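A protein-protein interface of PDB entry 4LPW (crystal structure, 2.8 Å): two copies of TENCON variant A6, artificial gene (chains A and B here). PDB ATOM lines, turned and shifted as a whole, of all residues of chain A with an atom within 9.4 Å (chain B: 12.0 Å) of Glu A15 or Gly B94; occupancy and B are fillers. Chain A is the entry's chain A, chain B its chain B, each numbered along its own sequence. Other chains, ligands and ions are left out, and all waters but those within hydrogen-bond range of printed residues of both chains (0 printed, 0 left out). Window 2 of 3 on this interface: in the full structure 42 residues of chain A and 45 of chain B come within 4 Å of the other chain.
OG1 of Thr B92 sits at hydrogen-bond distance from N of Thr A66. O of Lys A63 sits at hydrogen-bond distance from OG1 of Thr B92 (2.5 Å). The backbone NH (N) of Gly A65 sits at hydrogen-bond distance from the side-chain hydroxyl (OG1) of Thr B92, at 2.9 Å. N of Gly B93 is in hydrogen-bond range of O of Thr A14, 3.3 Å away. O of Phe B90 lies within hydrogen-bond range of N of Tyr A68, 2.8 Å away. The backbone NH (N) of Gly A65 sits at hydrogen-bond distance from the backbone carbonyl oxygen (O) of Gly B93 (2.9 Å). The backbone carbonyl oxygen of Gly B94 sits at hydrogen-bond distance from the backbone NH of Gly A65 (3.2 Å).
The side-chain hydroxyl of Thr A66 lies close to the backbone carbonyl oxygen of Lys A63 (3.4 Å). The side-chain hydroxyl (OG1) of Thr A14 is in hydrogen-bond range of the backbone NH (N) of Asp A16, 3.0 Å away. N of Ser A17 is in hydrogen-bond range of OG1 of Thr A14, at 2.8 Å. OH of Tyr A68 is in hydrogen-bond range of N of Lys A63 (2.8 Å). The backbone carbonyl oxygen (O) of Asp A16 lies within hydrogen-bond range of the backbone NH (N) of Leu A62 (3.0 Å). The side-chain hydroxyl (OG1) of Thr A66 sits at hydrogen-bond distance from the backbone carbonyl oxygen (O) of Pro A64.
Thr B91 touches Val A13 (O to CG1, 3.4 Å). Thr A14 touches Thr B92. Glu A15 touches Thr B92. Gly B93 touches Glu A15 (O to CG, 3.4 Å). Glu A15 touches Gly B94. CG2 of Thr B92 touches CD1 of Leu A62, 3.95 Å away. Gly B94 touches Pro A64. Thr B91 touches Thr A66. CA of Glu A67 touches O of Phe B90, 3.6 Å away. Glu A67 touches Thr B91 (CB to OG1, 3.4 Å).
Of chain B, only Thr B92 (3.1 Å), Gly B93 (3.4 Å) and Gly B94 (3.7 Å) come within 4 Å of Glu A15. Gly B94 touches just these residues of chain A: Glu A15, Pro A64 and Gly A65. Thr A14 touches just these residues of chain B: Thr B92 (3.5 Å) and Gly B93 (3.3 Å). Asp A16 touches none of the printed residues of chain B. No residue of chain B comes within 4 Å of Gly A61. Of the printed residues of chain B, Leu A62 touches Thr B92. Printed residues of chain B within 4 Å of Pro A64: Thr B92, Gly B93 and Gly B94. Gly A65 touches just these residues of chain B: Thr B92 (2.9 Å), Gly B93 (2.9 Å) and Gly B94 (3.2 Å). Gly B93 touches just these residues of chain A: Thr A14, Glu A15, Pro A64 and Gly A65. Of the printed residues of chain B, Glu A67 touches Phe B90 and Thr B91. Of the printed residues of chain A, Thr B91 touches Val A13, Thr A66 and Glu A67. Printed residues of chain A within 4 Å of Phe B90: Glu A67 (3.6 Å) and Tyr A68 (2.8 Å). Of the printed residues of chain B, Thr A66 touches Thr B91 and Thr B92. The nearest residue of chain B that does not touch Glu A15 is His B95 (5.3 Å). The nearest residue of chain A that does not touch Gly B94 is Thr A66 (5.9 Å).
Printed residues of chain A that touch a printed residue of chain B: Val A13, Thr A14, Glu A15, Leu A62, Lys A63, Pro A64, Gly A65, Thr A66, Glu A67 and Tyr A68. Hydrophobic or aromatic side chains of chain A within 4 Å of the printed part of chain B: Val A13, Leu A62, Pro A64 and Tyr A68. Among the printed residues, no Asp or Glu carboxylate lies within 4 Å of a Lys or Arg side-chain nitrogen of the other chain.
No position is printed for both chains.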
ATOM      1  N   GLU A  12      29.234 -36.936   3.874  1.00  0.00           N
ATOM      2  CA  GLU A  12      28.643 -35.883   4.709  1.00  0.00           C
ATOM      3  C   GLU A  12      27.735 -34.920   3.932  1.00  0.00           C
ATOM      4  O   GLU A  12      27.731 -33.706   4.159  1.00  0.00           O
ATOM      5  CB  GLU A  12      29.725 -35.137   5.496  1.00  0.00           C
ATOM      6  CG  GLU A  12      30.583 -36.062   6.335  1.00  0.00           C
ATOM      7  CD  GLU A  12      31.523 -35.319   7.268  1.00  0.00           C
ATOM      8  OE1 GLU A  12      32.329 -35.987   7.954  1.00  0.00           O
ATOM      9  OE2 GLU A  12      31.452 -34.068   7.313  1.00  0.00           O
ATOM     10  N   VAL A  13      26.952 -35.501   3.030  1.00  0.00           N
ATOM     11  CA  VAL A  13      25.979 -34.782   2.211  1.00  0.00           C
ATOM     12  C   VAL A  13      24.857 -34.151   3.022  1.00  0.00           C
ATOM     13  O   VAL A  13      23.884 -34.820   3.359  1.00  0.00           O
ATOM     14  CB  VAL A  13      25.316 -35.752   1.216  1.00  0.00           C
ATOM     15  CG1 VAL A  13      24.551 -35.001   0.158  1.00  0.00           C
ATOM     16  CG2 VAL A  13      26.366 -36.655   0.570  1.00  0.00           C
ATOM     17  N   THR A  14      24.990 -32.864   3.333  1.00  0.00           N
ATOM     18  CA  THR A  14      23.898 -32.103   3.941  1.00  0.00           C
ATOM     19  C   THR A  14      23.299 -31.158   2.906  1.00  0.00           C
ATOM     20  O   THR A  14      23.712 -31.171   1.746  1.00  0.00           O
ATOM     21  CB  THR A  14      24.382 -31.264   5.112  1.00  0.00           C
ATOM     22  OG1 THR A  14      24.936 -30.041   4.613  1.00  0.00           O
ATOM     23  CG2 THR A  14      25.429 -32.030   5.894  1.00  0.00           C
ATOM     24  N   GLU A  15      22.342 -30.333   3.325  1.00  0.00           N
ATOM     25  CA  GLU A  15      21.742 -29.357   2.424  1.00  0.00           C
ATOM     26  C   GLU A  15      22.767 -28.313   2.039  1.00  0.00           C
ATOM     27  O   GLU A  15      22.825 -27.901   0.893  1.00  0.00           O
ATOM     28  CB  GLU A  15      20.518 -28.679   3.050  1.00  0.00           C
ATOM     29  CG  GLU A  15      19.420 -29.633   3.516  1.00  0.00           C
ATOM     30  CD  GLU A  15      18.099 -28.930   3.833  1.00  0.00           C
ATOM     31  OE1 GLU A  15      18.117 -27.713   4.114  1.00  0.00           O
ATOM     32  OE2 GLU A  15      17.040 -29.596   3.788  1.00  0.00           O
ATOM     33  N   ASP A  16      23.584 -27.893   2.995  1.00  0.00           N
ATOM     34  CA  ASP A  16      24.499 -26.781   2.756  1.00  0.00           C
ATOM     35  C   ASP A  16      25.992 -27.153   2.702  1.00  0.00           C
ATOM     36  O   ASP A  16      26.850 -26.264   2.636  1.00  0.00           O
ATOM     37  CB  ASP A  16      24.267 -25.663   3.781  1.00  0.00           C
ATOM     38  CG  ASP A  16      24.747 -26.036   5.183  1.00  0.00           C
ATOM     39  OD1 ASP A  16      25.962 -25.897   5.465  1.00  0.00           O
ATOM     40  OD2 ASP A  16      23.908 -26.451   6.014  1.00  0.00           O
ATOM     41  N   SER A  17      26.312 -28.445   2.718  1.00  0.00           N
ATOM     42  CA  SER A  17      27.715 -28.849   2.756  1.00  0.00           C
ATOM     43  C   SER A  17      28.015 -30.206   2.126  1.00  0.00           C
ATOM     44  O   SER A  17      27.185 -31.111   2.142  1.00  0.00           O
ATOM     45  CB  SER A  17      28.237 -28.840   4.197  1.00  0.00           C
ATOM     46  OG  SER A  17      27.766 -29.964   4.920  1.00  0.00           O
ATOM     47  N   LEU A  18      29.227 -30.337   1.598  1.00  0.00           N
ATOM     48  CA  LEU A  18      29.721 -31.586   1.029  1.00  0.00           C
ATOM     49  C   LEU A  18      31.185 -31.748   1.394  1.00  0.00           C
ATOM     50  O   LEU A  18      31.968 -30.818   1.210  1.00  0.00           O
ATOM     51  CB  LEU A  18      29.637 -31.535  -0.491  1.00  0.00           C
ATOM     52  CG  LEU A  18      28.260 -31.504  -1.128  1.00  0.00           C
ATOM     53  CD1 LEU A  18      28.396 -31.111  -2.590  1.00  0.00           C
ATOM     54  CD2 LEU A  18      27.627 -32.878  -0.976  1.00  0.00           C
ATOM     55  N   LEU A  59      33.217 -28.528   1.536  1.00  0.00           N
ATOM     56  CA  LEU A  59      32.574 -27.391   0.893  1.00  0.00           C
ATOM     57  C   LEU A  59      31.408 -26.904   1.746  1.00  0.00           C
ATOM     58  O   LEU A  59      30.585 -27.695   2.212  1.00  0.00           O
ATOM     59  CB  LEU A  59      32.039 -27.802  -0.471  1.00  0.00           C
ATOM     60  CG  LEU A  59      32.847 -27.482  -1.723  1.00  0.00           C
ATOM     61  CD1 LEU A  59      34.318 -27.828  -1.542  1.00  0.00           C
ATOM     62  CD2 LEU A  59      32.254 -28.204  -2.931  1.00  0.00           C
ATOM     63  N   THR A  60      31.324 -25.596   1.945  1.00  0.00           N
ATOM     64  CA  THR A  60      30.261 -25.035   2.777  1.00  0.00           C
ATOM     65  C   THR A  60      29.495 -23.967   2.009  1.00  0.00           C
ATOM     66  O   THR A  60      29.866 -23.615   0.884  1.00  0.00           O
ATOM     67  CB  THR A  60      30.834 -24.396   4.048  1.00  0.00           C
ATOM     68  OG1 THR A  60      31.665 -23.292   3.676  1.00  0.00           O
ATOM     69  CG2 THR A  60      31.671 -25.407   4.829  1.00  0.00           C
ATOM     70  N   GLY A  61      28.442 -23.442   2.627  1.00  0.00           N
ATOM     71  CA  GLY A  61      27.713 -22.327   2.059  1.00  0.00           C
ATOM     72  C   GLY A  61      26.920 -22.702   0.828  1.00  0.00           C
ATOM     73  O   GLY A  61      26.603 -21.854  -0.014  1.00  0.00           O
ATOM     74  N   LEU A  62      26.572 -23.979   0.731  1.00  0.00           N
ATOM     75  CA  LEU A  62      25.917 -24.497  -0.466  1.00  0.00           C
ATOM     76  C   LEU A  62      24.399 -24.283  -0.432  1.00  0.00           C
ATOM     77  O   LEU A  62      23.863 -23.724   0.524  1.00  0.00           O
ATOM     78  CB  LEU A  62      26.261 -25.978  -0.646  1.00  0.00           C
ATOM     79  CG  LEU A  62      27.762 -26.325  -0.622  1.00  0.00           C
ATOM     80  CD1 LEU A  62      27.978 -27.833  -0.746  1.00  0.00           C
ATOM     81  CD2 LEU A  62      28.545 -25.589  -1.714  1.00  0.00           C
ATOM     82  N   LYS A  63      23.723 -24.713  -1.495  1.00  0.00           N
ATOM     83  CA  LYS A  63      22.273 -24.592  -1.604  1.00  0.00           C
ATOM     84  C   LYS A  63      21.619 -25.963  -1.549  1.00  0.00           C
ATOM     85  O   LYS A  63      22.162 -26.933  -2.064  1.00  0.00           O
ATOM     86  CB  LYS A  63      21.888 -23.850  -2.891  1.00  0.00           C
ATOM     87  CG  LYS A  63      22.166 -22.348  -2.814  1.00  0.00           C
ATOM     88  CD  LYS A  63      21.745 -21.598  -4.076  1.00  0.00           C
ATOM     89  CE  LYS A  63      21.641 -20.095  -3.800  1.00  0.00           C
ATOM     90  NZ  LYS A  63      20.512 -19.753  -2.870  1.00  0.00           N
ATOM     91  N   PRO A  64      20.454 -26.053  -0.904  1.00  0.00           N
ATOM     92  CA  PRO A  64      19.801 -27.353  -0.750  1.00  0.00           C
ATOM     93  C   PRO A  64      19.341 -27.916  -2.089  1.00  0.00           C
ATOM     94  O   PRO A  64      18.922 -27.164  -2.973  1.00  0.00           O
ATOM     95  CB  PRO A  64      18.591 -27.023   0.112  1.00  0.00           C
ATOM     96  CG  PRO A  64      19.005 -25.804   0.874  1.00  0.00           C
ATOM     97  CD  PRO A  64      19.801 -25.007  -0.103  1.00  0.00           C
ATOM     98  N   GLY A  65      19.440 -29.233  -2.237  1.00  0.00           N
ATOM     99  CA  GLY A  65      18.969 -29.920  -3.423  1.00  0.00           C
ATOM    100  C   GLY A  65      19.639 -29.516  -4.719  1.00  0.00           C
ATOM    101  O   GLY A  65      19.086 -29.783  -5.786  1.00  0.00           O
ATOM    102  N   THR A  66      20.821 -28.900  -4.645  1.00  0.00           N
ATOM    103  CA  THR A  66      21.493 -28.400  -5.850  1.00  0.00           C
ATOM    104  C   THR A  66      22.681 -29.255  -6.283  1.00  0.00           C
ATOM    105  O   THR A  66      23.448 -29.741  -5.446  1.00  0.00           O
ATOM    106  CB  THR A  66      21.993 -26.963  -5.669  1.00  0.00           C
ATOM    107  OG1 THR A  66      20.929 -26.145  -5.186  1.00  0.00           O
ATOM    108  CG2 THR A  66      22.481 -26.394  -6.990  1.00  0.00           C
ATOM    109  N   GLU A  67      22.837 -29.420  -7.595  1.00  0.00           N
ATOM    110  CA  GLU A  67      23.959 -30.165  -8.145  1.00  0.00           C
ATOM    111  C   GLU A  67      25.117 -29.243  -8.539  1.00  0.00           C
ATOM    112  O   GLU A  67      24.925 -28.226  -9.213  1.00  0.00           O
ATOM    113  CB  GLU A  67      23.511 -30.986  -9.348  1.00  0.00           C
ATOM    114  CG  GLU A  67      24.622 -31.715 -10.056  1.00  0.00           C
ATOM    115  CD  GLU A  67      24.159 -32.256 -11.392  1.00  0.00           C
ATOM    116  OE1 GLU A  67      22.940 -32.495 -11.529  1.00  0.00           O
ATOM    117  OE2 GLU A  67      24.995 -32.421 -12.307  1.00  0.00           O
ATOM    118  N   TYR A  68      26.319 -29.639  -8.122  1.00  0.00           N
ATOM    119  CA  TYR A  68      27.525 -28.840  -8.253  1.00  0.00           C
ATOM    120  C   TYR A  68      28.592 -29.607  -8.987  1.00  0.00           C
ATOM    121  O   TYR A  68      28.996 -30.681  -8.542  1.00  0.00           O
ATOM    122  CB  TYR A  68      28.087 -28.507  -6.870  1.00  0.00           C
ATOM    123  CG  TYR A  68      27.267 -27.524  -6.095  1.00  0.00           C
ATOM    124  CD1 TYR A  68      26.111 -27.915  -5.441  1.00  0.00           C
ATOM    125  CD2 TYR A  68      27.642 -26.201  -6.018  1.00  0.00           C
ATOM    126  CE1 TYR A  68      25.350 -27.008  -4.732  1.00  0.00           C
ATOM    127  CE2 TYR A  68      26.894 -25.290  -5.306  1.00  0.00           C
ATOM    128  CZ  TYR A  68      25.747 -25.699  -4.667  1.00  0.00           C
ATOM    129  OH  TYR A  68      25.007 -24.787  -3.958  1.00  0.00           O
ATOM    130  N   PHE B  90      28.368 -33.592  -7.801  1.00  0.00           N
ATOM    131  CA  PHE B  90      27.810 -33.973  -6.515  1.00  0.00           C
ATOM    132  C   PHE B  90      26.663 -33.041  -6.154  1.00  0.00           C
ATOM    133  O   PHE B  90      26.697 -31.862  -6.490  1.00  0.00           O
ATOM    134  CB  PHE B  90      28.903 -33.965  -5.448  1.00  0.00           C
ATOM    135  CG  PHE B  90      30.012 -34.948  -5.713  1.00  0.00           C
ATOM    136  CD1 PHE B  90      29.733 -36.202  -6.218  1.00  0.00           C
ATOM    137  CD2 PHE B  90      31.334 -34.612  -5.476  1.00  0.00           C
ATOM    138  CE1 PHE B  90      30.738 -37.102  -6.455  1.00  0.00           C
ATOM    139  CE2 PHE B  90      32.348 -35.519  -5.718  1.00  0.00           C
ATOM    140  CZ  PHE B  90      32.041 -36.765  -6.204  1.00  0.00           C
ATOM    141  N   THR B  91      25.655 -33.572  -5.467  1.00  0.00           N
ATOM    142  CA  THR B  91      24.404 -32.861  -5.234  1.00  0.00           C
ATOM    143  C   THR B  91      24.049 -32.839  -3.742  1.00  0.00           C
ATOM    144  O   THR B  91      24.158 -33.859  -3.061  1.00  0.00           O
ATOM    145  CB  THR B  91      23.255 -33.537  -6.008  1.00  0.00           C
ATOM    146  OG1 THR B  91      23.670 -33.777  -7.357  1.00  0.00           O
ATOM    147  CG2 THR B  91      22.002 -32.663  -6.011  1.00  0.00           C
ATOM    148  N   THR B  92      23.618 -31.679  -3.240  1.00  0.00           N
ATOM    149  CA  THR B  92      23.192 -31.524  -1.841  1.00  0.00           C
ATOM    150  C   THR B  92      21.838 -32.197  -1.585  1.00  0.00           C
ATOM    151  O   THR B  92      21.123 -32.557  -2.527  1.00  0.00           O
ATOM    152  CB  THR B  92      23.046 -30.043  -1.462  1.00  0.00           C
ATOM    153  OG1 THR B  92      22.335 -29.357  -2.502  1.00  0.00           O
ATOM    154  CG2 THR B  92      24.397 -29.419  -1.266  1.00  0.00           C
ATOM    155  N   GLY B  93      21.463 -32.337  -0.315  1.00  0.00           N
ATOM    156  CA  GLY B  93      20.181 -32.931   0.021  1.00  0.00           C
ATOM    157  C   GLY B  93      19.063 -31.916   0.234  1.00  0.00           C
ATOM    158  O   GLY B  93      19.307 -30.710   0.282  1.00  0.00           O
ATOM    159  N   GLY B  94      17.830 -32.412   0.348  1.00  0.00           N
ATOM    160  CA  GLY B  94      16.687 -31.593   0.720  1.00  0.00           C
ATOM    161  C   GLY B  94      16.185 -30.570  -0.286  1.00  0.00           C
ATOM    162  O   GLY B  94      16.772 -29.503  -0.447  1.00  0.00           O
ATOM    163  N   HIS B  95      15.072 -30.880  -0.945  1.00  0.00           N
ATOM    164  CA  HIS B  95      14.388 -29.909  -1.796  1.00  0.00           C
ATOM    165  C   HIS B  95      12.882 -30.183  -1.815  1.00  0.00           C
ATOM    166  O   HIS B  95      12.392 -31.092  -1.140  1.00  0.00           O
ATOM    167  CB  HIS B  95      14.951 -29.929  -3.218  1.00  0.00           C
ATOM    168  CG  HIS B  95      14.910 -28.605  -3.915  1.00  0.00           C
ATOM    169  ND1 HIS B  95      14.812 -27.409  -3.217  1.00  0.00           N
ATOM    170  CD2 HIS B  95      14.956 -28.272  -5.218  1.00  0.00           C
ATOM    171  CE1 HIS B  95      14.805 -26.407  -4.083  1.00  0.00           C
ATOM    172  NE2 HIS B  95      14.892 -26.900  -5.301  1.00  0.00           N
